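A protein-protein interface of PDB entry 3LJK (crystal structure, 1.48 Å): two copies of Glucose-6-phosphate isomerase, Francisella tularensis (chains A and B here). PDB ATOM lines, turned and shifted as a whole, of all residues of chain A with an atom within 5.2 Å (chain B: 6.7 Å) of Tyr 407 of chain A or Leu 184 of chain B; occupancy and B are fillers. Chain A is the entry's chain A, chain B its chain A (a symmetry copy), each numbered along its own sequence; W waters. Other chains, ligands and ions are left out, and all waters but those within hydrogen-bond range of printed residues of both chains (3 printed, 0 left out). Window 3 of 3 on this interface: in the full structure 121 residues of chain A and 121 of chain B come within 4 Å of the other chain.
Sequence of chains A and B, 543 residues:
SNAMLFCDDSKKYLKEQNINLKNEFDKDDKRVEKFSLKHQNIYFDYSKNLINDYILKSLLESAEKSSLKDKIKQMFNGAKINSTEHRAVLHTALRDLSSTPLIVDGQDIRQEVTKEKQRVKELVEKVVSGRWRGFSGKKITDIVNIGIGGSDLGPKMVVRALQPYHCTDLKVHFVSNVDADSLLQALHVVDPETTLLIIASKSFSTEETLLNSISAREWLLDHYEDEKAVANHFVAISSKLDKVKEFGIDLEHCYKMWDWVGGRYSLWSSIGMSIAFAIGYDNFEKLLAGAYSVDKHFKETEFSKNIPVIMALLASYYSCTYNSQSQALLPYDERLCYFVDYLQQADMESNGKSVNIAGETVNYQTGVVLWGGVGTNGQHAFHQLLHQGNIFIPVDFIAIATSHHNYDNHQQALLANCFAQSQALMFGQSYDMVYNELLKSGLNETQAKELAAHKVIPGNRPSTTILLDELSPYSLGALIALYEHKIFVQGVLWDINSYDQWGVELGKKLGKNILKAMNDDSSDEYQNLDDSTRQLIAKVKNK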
ATOM      1  N   HIS A 404     -16.986  27.256 -14.293  1.00  0.00           N
ATOM      2  CA  HIS A 404     -17.073  27.945 -15.571  1.00  0.00           C
ATOM      3  C   HIS A 404     -15.996  27.534 -16.554  1.00  0.00           C
ATOM      4  O   HIS A 404     -15.660  28.274 -17.464  1.00  0.00           O
ATOM      5  CB  HIS A 404     -17.035  29.464 -15.338  1.00  0.00           C
ATOM      6  CG  HIS A 404     -15.725  29.962 -14.812  1.00  0.00           C
ATOM      7  ND1 HIS A 404     -14.760  30.503 -15.627  1.00  0.00           N
ATOM      8  CD2 HIS A 404     -15.225  30.015 -13.548  1.00  0.00           C
ATOM      9  CE1 HIS A 404     -13.710  30.847 -14.884  1.00  0.00           C
ATOM     10  NE2 HIS A 404     -13.962  30.545 -13.623  1.00  0.00           N
ATOM     11  N   HIS A 405     -15.421  26.368 -16.367  1.00  0.00           N
ATOM     12  CA  HIS A 405     -14.322  25.854 -17.178  1.00  0.00           C
ATOM     13  C   HIS A 405     -14.447  24.341 -17.278  1.00  0.00           C
ATOM     14  O   HIS A 405     -15.323  23.717 -16.638  1.00  0.00           O
ATOM     15  CB  HIS A 405     -12.989  26.230 -16.509  1.00  0.00           C
ATOM     16  CG  HIS A 405     -12.872  25.670 -15.124  1.00  0.00           C
ATOM     17  ND1 HIS A 405     -12.658  24.321 -14.919  1.00  0.00           N
ATOM     18  CD2 HIS A 405     -13.073  26.217 -13.894  1.00  0.00           C
ATOM     19  CE1 HIS A 405     -12.676  24.070 -13.623  1.00  0.00           C
ATOM     20  NE2 HIS A 405     -12.927  25.204 -12.972  1.00  0.00           N
ATOM     21  N   ASN A 406     -13.533  23.744 -18.037  1.00  0.00           N
ATOM     22  CA  ASN A 406     -13.560  22.297 -18.277  1.00  0.00           C
ATOM     23  C   ASN A 406     -12.411  21.505 -17.645  1.00  0.00           C
ATOM     24  O   ASN A 406     -12.096  20.352 -18.049  1.00  0.00           O
ATOM     25  CB  ASN A 406     -13.612  22.026 -19.765  1.00  0.00           C
ATOM     26  CG  ASN A 406     -14.955  22.471 -20.380  1.00  0.00           C
ATOM     27  OD1 ASN A 406     -16.008  22.116 -19.864  1.00  0.00           O
ATOM     28  ND2 ASN A 406     -14.903  23.299 -21.395  1.00  0.00           N
ATOM     29  N   TYR A 407     -11.819  22.089 -16.605  1.00  0.00           N
ATOM     30  CA  TYR A 407     -10.805  21.354 -15.777  1.00  0.00           C
ATOM     31  C   TYR A 407     -11.562  20.507 -14.740  1.00  0.00           C
ATOM     32  O   TYR A 407     -11.601  20.802 -13.547  1.00  0.00           O
ATOM     33  CB  TYR A 407      -9.820  22.328 -15.126  1.00  0.00           C
ATOM     34  CG  TYR A 407      -8.830  22.919 -16.068  1.00  0.00           C
ATOM     35  CD1 TYR A 407      -7.568  22.375 -16.189  1.00  0.00           C
ATOM     36  CD2 TYR A 407      -9.128  24.016 -16.829  1.00  0.00           C
ATOM     37  CE1 TYR A 407      -6.637  22.916 -16.994  1.00  0.00           C
ATOM     38  CE2 TYR A 407      -8.193  24.569 -17.688  1.00  0.00           C
ATOM     39  CZ  TYR A 407      -6.938  24.014 -17.750  1.00  0.00           C
ATOM     40  OH  TYR A 407      -5.982  24.510 -18.566  1.00  0.00           O
ATOM     41  N   ASP A 408     -12.207  19.463 -15.239  1.00  0.00           N
ATOM     42  CA  ASP A 408     -13.136  18.698 -14.443  1.00  0.00           C
ATOM     43  C   ASP A 408     -12.441  18.018 -13.263  1.00  0.00           C
ATOM     44  O   ASP A 408     -13.057  17.871 -12.193  1.00  0.00           O
ATOM     45  CB  ASP A 408     -13.851  17.663 -15.285  1.00  0.00           C
ATOM     46  CG  ASP A 408     -14.799  18.286 -16.322  1.00  0.00           C
ATOM     47  OD1 ASP A 408     -15.148  19.464 -16.224  1.00  0.00           O
ATOM     48  OD2 ASP A 408     -15.200  17.531 -17.205  1.00  0.00           O
ATOM     49  N   ASN A 409     -11.158  17.645 -13.429  1.00  0.00           N
ATOM     50  CA  ASN A 409     -10.419  17.040 -12.323  1.00  0.00           C
ATOM     51  C   ASN A 409     -10.207  18.016 -11.172  1.00  0.00           C
ATOM     52  O   ASN A 409     -10.305  17.623 -10.011  1.00  0.00           O
ATOM     53  CB  ASN A 409      -9.099  16.448 -12.794  1.00  0.00           C
ATOM     54  CG  ASN A 409      -8.152  17.450 -13.361  1.00  0.00           C
ATOM     55  OD1 ASN A 409      -8.548  18.417 -14.063  1.00  0.00           O
ATOM     56  ND2 ASN A 409      -6.859  17.251 -13.032  1.00  0.00           N
ATOM     57  N   HIS A 410      -9.975  19.283 -11.498  1.00  0.00           N
ATOM     58  CA  HIS A 410      -9.823  20.284 -10.475  1.00  0.00           C
ATOM     59  C   HIS A 410     -11.143  20.488  -9.723  1.00  0.00           C
ATOM     60  O   HIS A 410     -11.162  20.608  -8.505  1.00  0.00           O
ATOM     61  CB  HIS A 410      -9.391  21.629 -11.064  1.00  0.00           C
ATOM     62  CG  HIS A 410      -7.965  21.693 -11.484  1.00  0.00           C
ATOM     63  ND1 HIS A 410      -7.059  22.502 -10.843  1.00  0.00           N
ATOM     64  CD2 HIS A 410      -7.296  21.117 -12.527  1.00  0.00           C
ATOM     65  CE1 HIS A 410      -5.885  22.401 -11.463  1.00  0.00           C
ATOM     66  NE2 HIS A 410      -5.994  21.556 -12.470  1.00  0.00           N
ATOM     67  N   GLN A 411     -12.247  20.587 -10.455  1.00  0.00           N
ATOM     68  CA  GLN A 411     -13.558  20.814  -9.824  1.00  0.00           C
ATOM     69  C   GLN A 411     -13.953  19.643  -8.918  1.00  0.00           C
ATOM     70  O   GLN A 411     -14.455  19.850  -7.823  1.00  0.00           O
ATOM     71  CB  GLN A 411     -14.577  21.070 -10.902  1.00  0.00           C
ATOM     72  CG  GLN A 411     -15.941  21.362 -10.362  1.00  0.00           C
ATOM     73  CD  GLN A 411     -16.104  22.708  -9.620  1.00  0.00           C
ATOM     74  OE1 GLN A 411     -15.203  23.553  -9.626  1.00  0.00           O
ATOM     75  NE2 GLN A 411     -17.278  22.907  -8.997  1.00  0.00           N
ATOM     76  N   VAL B 175      -0.886  31.383  -7.965  1.00  0.00           N
ATOM     77  CA  VAL B 175      -1.838  30.310  -8.217  1.00  0.00           C
ATOM     78  C   VAL B 175      -1.778  29.413  -6.986  1.00  0.00           C
ATOM     79  O   VAL B 175      -0.676  29.053  -6.550  1.00  0.00           O
ATOM     80  CB  VAL B 175      -1.474  29.540  -9.485  1.00  0.00           C
ATOM     81  CG1 VAL B 175      -2.283  28.240  -9.632  1.00  0.00           C
ATOM     82  CG2 VAL B 175      -1.552  30.459 -10.720  1.00  0.00           C
ATOM     83  N   VAL B 178      -6.949  24.620  -5.606  1.00  0.00           N
ATOM     84  CA  VAL B 178      -7.209  23.631  -6.636  1.00  0.00           C
ATOM     85  C   VAL B 178      -8.349  24.067  -7.563  1.00  0.00           C
ATOM     86  O   VAL B 178      -8.375  23.668  -8.709  1.00  0.00           O
ATOM     87  CB  VAL B 178      -7.481  22.232  -6.055  1.00  0.00           C
ATOM     88  CG1 VAL B 178      -8.761  22.165  -5.230  1.00  0.00           C
ATOM     89  CG2 VAL B 178      -7.403  21.164  -7.124  1.00  0.00           C
ATOM     90  N   ASP B 179      -9.275  24.903  -7.085  1.00  0.00           N
ATOM     91  CA  ASP B 179     -10.287  25.523  -7.952  1.00  0.00           C
ATOM     92  C   ASP B 179      -9.544  26.114  -9.140  1.00  0.00           C
ATOM     93  O   ASP B 179      -8.735  27.023  -8.963  1.00  0.00           O
ATOM     94  CB  ASP B 179     -10.994  26.651  -7.181  1.00  0.00           C
ATOM     95  CG  ASP B 179     -12.044  27.399  -7.989  1.00  0.00           C
ATOM     96  OD1 ASP B 179     -12.226  27.108  -9.194  1.00  0.00           O
ATOM     97  OD2 ASP B 179     -12.698  28.261  -7.371  1.00  0.00           O
ATOM     98  N   ALA B 180      -9.828  25.615 -10.346  1.00  0.00           N
ATOM     99  CA  ALA B 180      -9.065  26.000 -11.526  1.00  0.00           C
ATOM    100  C   ALA B 180      -9.200  27.486 -11.868  1.00  0.00           C
ATOM    101  O   ALA B 180      -8.434  28.016 -12.687  1.00  0.00           O
ATOM    102  CB  ALA B 180      -9.383  25.114 -12.736  1.00  0.00           C
ATOM    103  N   ASP B 181     -10.191  28.154 -11.309  1.00  0.00           N
ATOM    104  CA  ASP B 181     -10.231  29.610 -11.474  1.00  0.00           C
ATOM    105  C   ASP B 181      -8.877  30.242 -11.083  1.00  0.00           C
ATOM    106  O   ASP B 181      -8.475  31.204 -11.707  1.00  0.00           O
ATOM    107  CB  ASP B 181     -11.369  30.204 -10.633  1.00  0.00           C
ATOM    108  CG  ASP B 181     -11.623  31.664 -10.915  1.00  0.00           C
ATOM    109  OD1 ASP B 181     -12.322  31.891 -11.915  1.00  0.00           O
ATOM    110  OD2 ASP B 181     -11.166  32.520 -10.157  1.00  0.00           O
ATOM    111  N   SER B 182      -8.202  29.747 -10.047  1.00  0.00           N
ATOM    112  CA  SER B 182      -6.915  30.306  -9.635  1.00  0.00           C
ATOM    113  C   SER B 182      -5.867  30.197 -10.747  1.00  0.00           C
ATOM    114  O   SER B 182      -5.246  31.200 -11.162  1.00  0.00           O
ATOM    115  CB  SER B 182      -6.418  29.652  -8.360  1.00  0.00           C
ATOM    116  OG  SER B 182      -5.261  30.304  -7.871  1.00  0.00           O
ATOM    117  N   LEU B 183      -5.661  29.001 -11.247  1.00  0.00           N
ATOM    118  CA  LEU B 183      -4.715  28.796 -12.362  1.00  0.00           C
ATOM    119  C   LEU B 183      -5.100  29.646 -13.578  1.00  0.00           C
ATOM    120  O   LEU B 183      -4.235  30.302 -14.205  1.00  0.00           O
ATOM    121  CB  LEU B 183      -4.632  27.316 -12.752  1.00  0.00           C
ATOM    122  CG  LEU B 183      -3.740  26.966 -13.943  1.00  0.00           C
ATOM    123  CD1 LEU B 183      -2.296  27.312 -13.686  1.00  0.00           C
ATOM    124  CD2 LEU B 183      -3.930  25.457 -14.273  1.00  0.00           C
ATOM    125  N   LEU B 184      -6.395  29.679 -13.909  1.00  0.00           N
ATOM    126  CA  LEU B 184      -6.867  30.382 -15.080  1.00  0.00           C
ATOM    127  C   LEU B 184      -6.665  31.863 -15.011  1.00  0.00           C
ATOM    128  O   LEU B 184      -6.422  32.491 -16.042  1.00  0.00           O
ATOM    129  CB  LEU B 184      -8.327  30.032 -15.384  1.00  0.00           C
ATOM    130  CG  LEU B 184      -8.495  28.596 -15.926  1.00  0.00           C
ATOM    131  CD1 LEU B 184      -9.975  28.152 -15.913  1.00  0.00           C
ATOM    132  CD2 LEU B 184      -7.908  28.414 -17.296  1.00  0.00           C
ATOM    133  N   GLN B 185      -6.744  32.440 -13.821  1.00  0.00           N
ATOM    134  CA  GLN B 185      -6.522  33.891 -13.741  1.00  0.00           C
ATOM    135  C   GLN B 185      -5.118  34.247 -14.162  1.00  0.00           C
ATOM    136  O   GLN B 185      -4.895  35.323 -14.721  1.00  0.00           O
ATOM    137  CB  GLN B 185      -6.780  34.479 -12.357  1.00  0.00           C
ATOM    138  CG  GLN B 185      -8.186  34.387 -11.838  1.00  0.00           C
ATOM    139  CD  GLN B 185      -9.188  34.775 -12.865  1.00  0.00           C
ATOM    140  OE1 GLN B 185      -9.194  35.940 -13.324  1.00  0.00           O
ATOM    141  NE2 GLN B 185     -10.007  33.795 -13.318  1.00  0.00           N
ATOM    142  N   ALA B 186      -4.163  33.365 -13.879  1.00  0.00           N
ATOM    143  CA  ALA B 186      -2.795  33.568 -14.358  1.00  0.00           C
ATOM    144  C   ALA B 186      -2.676  33.235 -15.822  1.00  0.00           C
ATOM    145  O   ALA B 186      -2.161  34.050 -16.613  1.00  0.00           O
ATOM    146  CB  ALA B 186      -1.823  32.690 -13.489  1.00  0.00           C
ATOM    147  N   LEU B 187      -3.106  32.044 -16.226  1.00  0.00           N
ATOM    148  CA  LEU B 187      -2.913  31.617 -17.606  1.00  0.00           C
ATOM    149  C   LEU B 187      -3.573  32.539 -18.622  1.00  0.00           C
ATOM    150  O   LEU B 187      -3.068  32.716 -19.736  1.00  0.00           O
ATOM    151  CB  LEU B 187      -3.352  30.150 -17.827  1.00  0.00           C
ATOM    152  CG  LEU B 187      -2.625  29.103 -16.961  1.00  0.00           C
ATOM    153  CD1 LEU B 187      -3.062  27.720 -17.384  1.00  0.00           C
ATOM    154  CD2 LEU B 187      -1.068  29.228 -16.961  1.00  0.00           C
ATOM    155  N   HIS B 188      -4.682  33.162 -18.260  1.00  0.00           N
ATOM    156  CA  HIS B 188      -5.369  34.094 -19.178  1.00  0.00           C
ATOM    157  C   HIS B 188      -4.553  35.302 -19.578  1.00  0.00           C
ATOM    158  O   HIS B 188      -4.841  35.921 -20.612  1.00  0.00           O
ATOM    159  CB  HIS B 188      -6.701  34.584 -18.560  1.00  0.00           C
ATOM    160  CG  HIS B 188      -7.807  33.579 -18.576  1.00  0.00           C
ATOM    161  ND1 HIS B 188      -8.941  33.739 -17.791  1.00  0.00           N
ATOM    162  CD2 HIS B 188      -7.965  32.409 -19.236  1.00  0.00           C
ATOM    163  CE1 HIS B 188      -9.756  32.722 -18.011  1.00  0.00           C
ATOM    164  NE2 HIS B 188      -9.192  31.904 -18.883  1.00  0.00           N
ATOM    165  N   VAL B 189      -3.569  35.647 -18.775  1.00  0.00           N
ATOM    166  CA  VAL B 189      -2.799  36.890 -18.968  1.00  0.00           C
ATOM    167  C   VAL B 189      -1.296  36.689 -19.161  1.00  0.00           C
ATOM    168  O   VAL B 189      -0.536  37.674 -19.231  1.00  0.00           O
ATOM    169  CB  VAL B 189      -3.083  37.902 -17.824  1.00  0.00           C
ATOM    170  CG1 VAL B 189      -4.523  38.332 -17.813  1.00  0.00           C
ATOM    171  CG2 VAL B 189      -2.631  37.393 -16.452  1.00  0.00           C
ATOM    172  N   SER B 215      -1.368  20.716 -14.569  1.00  0.00           N
ATOM    173  CA  SER B 215      -2.151  21.451 -15.521  1.00  0.00           C
ATOM    174  C   SER B 215      -1.325  22.582 -16.167  1.00  0.00           C
ATOM    175  O   SER B 215      -1.466  22.822 -17.385  1.00  0.00           O
ATOM    176  CB  SER B 215      -3.429  21.998 -14.858  1.00  0.00           C
ATOM    177  OG  SER B 215      -4.307  20.975 -14.516  1.00  0.00           O
ATOM    178  N   ALA B 216      -0.438  23.213 -15.400  1.00  0.00           N
ATOM    179  CA  ALA B 216       0.463  24.234 -15.958  1.00  0.00           C
ATOM    180  C   ALA B 216       1.417  23.606 -16.973  1.00  0.00           C
ATOM    181  O   ALA B 216       1.699  24.174 -18.027  1.00  0.00           O
ATOM    182  CB  ALA B 216       1.209  24.954 -14.846  1.00  0.00           C
ATOM    183  N   GLU B 218       0.857  20.946 -18.742  1.00  0.00           N
ATOM    184  CA  GLU B 218       0.081  20.600 -19.936  1.00  0.00           C
ATOM    185  C   GLU B 218      -0.143  21.837 -20.808  1.00  0.00           C
ATOM    186  O   GLU B 218      -0.046  21.767 -22.028  1.00  0.00           O
ATOM    187  CB  GLU B 218      -1.228  19.920 -19.512  1.00  0.00           C
ATOM    188  CG  GLU B 218      -0.993  18.511 -19.064  1.00  0.00           C
ATOM    189  CD  GLU B 218      -2.209  17.838 -18.427  1.00  0.00           C
ATOM    190  OE1 GLU B 218      -3.253  18.518 -18.203  1.00  0.00           O
ATOM    191  OE2 GLU B 218      -2.086  16.621 -18.095  1.00  0.00           O
ATOM    192  N   TRP B 219      -0.413  22.989 -20.194  1.00  0.00           N
ATOM    193  CA  TRP B 219      -0.558  24.244 -20.918  1.00  0.00           C
ATOM    194  C   TRP B 219       0.716  24.595 -21.679  1.00  0.00           C
ATOM    195  O   TRP B 219       0.680  24.981 -22.844  1.00  0.00           O
ATOM    196  CB  TRP B 219      -0.940  25.353 -19.936  1.00  0.00           C
ATOM    197  CG  TRP B 219      -0.829  26.764 -20.363  1.00  0.00           C
ATOM    198  CD1 TRP B 219      -1.739  27.503 -21.052  1.00  0.00           C
ATOM    199  CD2 TRP B 219       0.227  27.651 -20.035  1.00  0.00           C
ATOM    200  NE1 TRP B 219      -1.312  28.781 -21.201  1.00  0.00           N
ATOM    201  CE2 TRP B 219      -0.101  28.920 -20.572  1.00  0.00           C
ATOM    202  CE3 TRP B 219       1.407  27.513 -19.313  1.00  0.00           C
ATOM    203  CZ2 TRP B 219       0.699  30.059 -20.380  1.00  0.00           C
ATOM    204  CZ3 TRP B 219       2.214  28.663 -19.125  1.00  0.00           C
ATOM    205  CH2 TRP B 219       1.865  29.903 -19.688  1.00  0.00           C
HETATM  206  O   HOH W   1      -3.903  18.138 -13.131  1.00  0.00           O
HETATM  207  O   HOH W   2     -12.788  24.653 -10.243  1.00  0.00           O
HETATM  208  O   HOH W   3      -3.761  22.845 -18.922  1.00  0.00           O
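A ring nitrogen (NE2) of His 404 of chain A lies within hydrogen-bond range of the side-chain carboxylate of Asp 181 of chain B (2.7 Å).
ND1 of His 410 of chain A lies within hydrogen-bond range of O of Val 178 of chain B (2.8 Å).
A ring nitrogen (NE2) of His 410 of chain A lies within hydrogen-bond range of the side-chain hydroxyl (OG) of Ser 215 of chain B (2.7 Å).
The backbone NH (N) of Tyr 407 of chain A lies within hydrogen-bond range of a ring nitrogen (ND1) of His 405 of chain A, 2.9 Å away.
The side-chain carboxylate (OD1) of Asp 179 of chain B lies close to the backbone NH (N) of Asp 181 of chain B (3.1 Å).
NE2 of Gln 185 of chain B lies within hydrogen-bond range of OD1 of Asp 181 of chain B (3.3 Å).
The backbone carbonyl oxygen (O) of Leu 184 of chain B lies close to a ring nitrogen (ND1) of His 188 of chain B (3.3 Å).
NE2 of His 405 of chain A touches CB of Ala 180 of chain B, at 3.6 Å.
CB of His 405 of chain A touches CD1 of Leu 184 of chain B, at 3.6 Å.
CB of Tyr 407 of chain A touches CB of Ala 180 of chain B, at 3.7 Å.
Tyr 407 of chain A touches Leu 184 of chain B (CE2 to CD2, 3.9 Å).
OG of Ser 215 of chain B touches CE1 of Tyr 407 of chain A, at 3.9 Å.
His 410 of chain A touches Ala 180 of chain B (CB to CB, 3.9 Å).
Printed residues of chain B within 4 Å of His 405 of chain A: Ala 180 (3.6 Å) and Leu 184 (3.6 Å).
Of the printed residues of chain A, Asp 181 of chain B touches His 404 (2.7 Å).
Leu 184 of chain B touches just these residues of chain A: His 405 and Tyr 407.
Of the printed residues of chain A, Ser 215 of chain B touches Tyr 407 (3.9 Å) and His 410 (2.7 Å).
The nearest residue of chain A that does not touch Leu 184 of chain B is His 404 of chain A (4.7 Å).
The nearest printed residue of chain A that does not touch Val 178 of chain B is Gln 411 of chain A (5.2 Å).
Printed residues of chain A that touch a printed residue of chain B: His 404, His 405, Tyr 407 and His 410.
Hydrophobic or aromatic side chains of chain A within 4 Å of the printed part of chain B: His 404, His 405, Tyr 407 and His 410.
Of the 17 printed residues of chain B, 5 touch a printed residue of chain A.
Printed residues of chain B that touch a printed residue of chain A: Val 178, Ala 180, Asp 181, Leu 184 and Ser 215.
Hydrophobic or aromatic side chains of chain B within 4 Å of the printed part of chain A: Val 178, Ala 180 and Leu 184.
Among the printed residues, 9 pairs touch across the chains.
No position is printed for both chains.
Water W2 lies within hydrogen-bond range of the side-chain amide oxygen (OE1) of Gln 411 of chain A, the side-chain carboxylate (OD1) of Asp 179 of chain B, a ring nitrogen (NE2) of His 405 of chain A and the backbone NH (N) of Ala 180 of chain B.
Water W3 lies within hydrogen-bond range of O of Ser 215 of chain B and OH of Tyr 407 of chain A.
Water W1 lies within hydrogen-bond range of ND2 of Asn 409 of chain A (3.1 Å) and OG of Ser 215 of chain B (3.2 Å).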
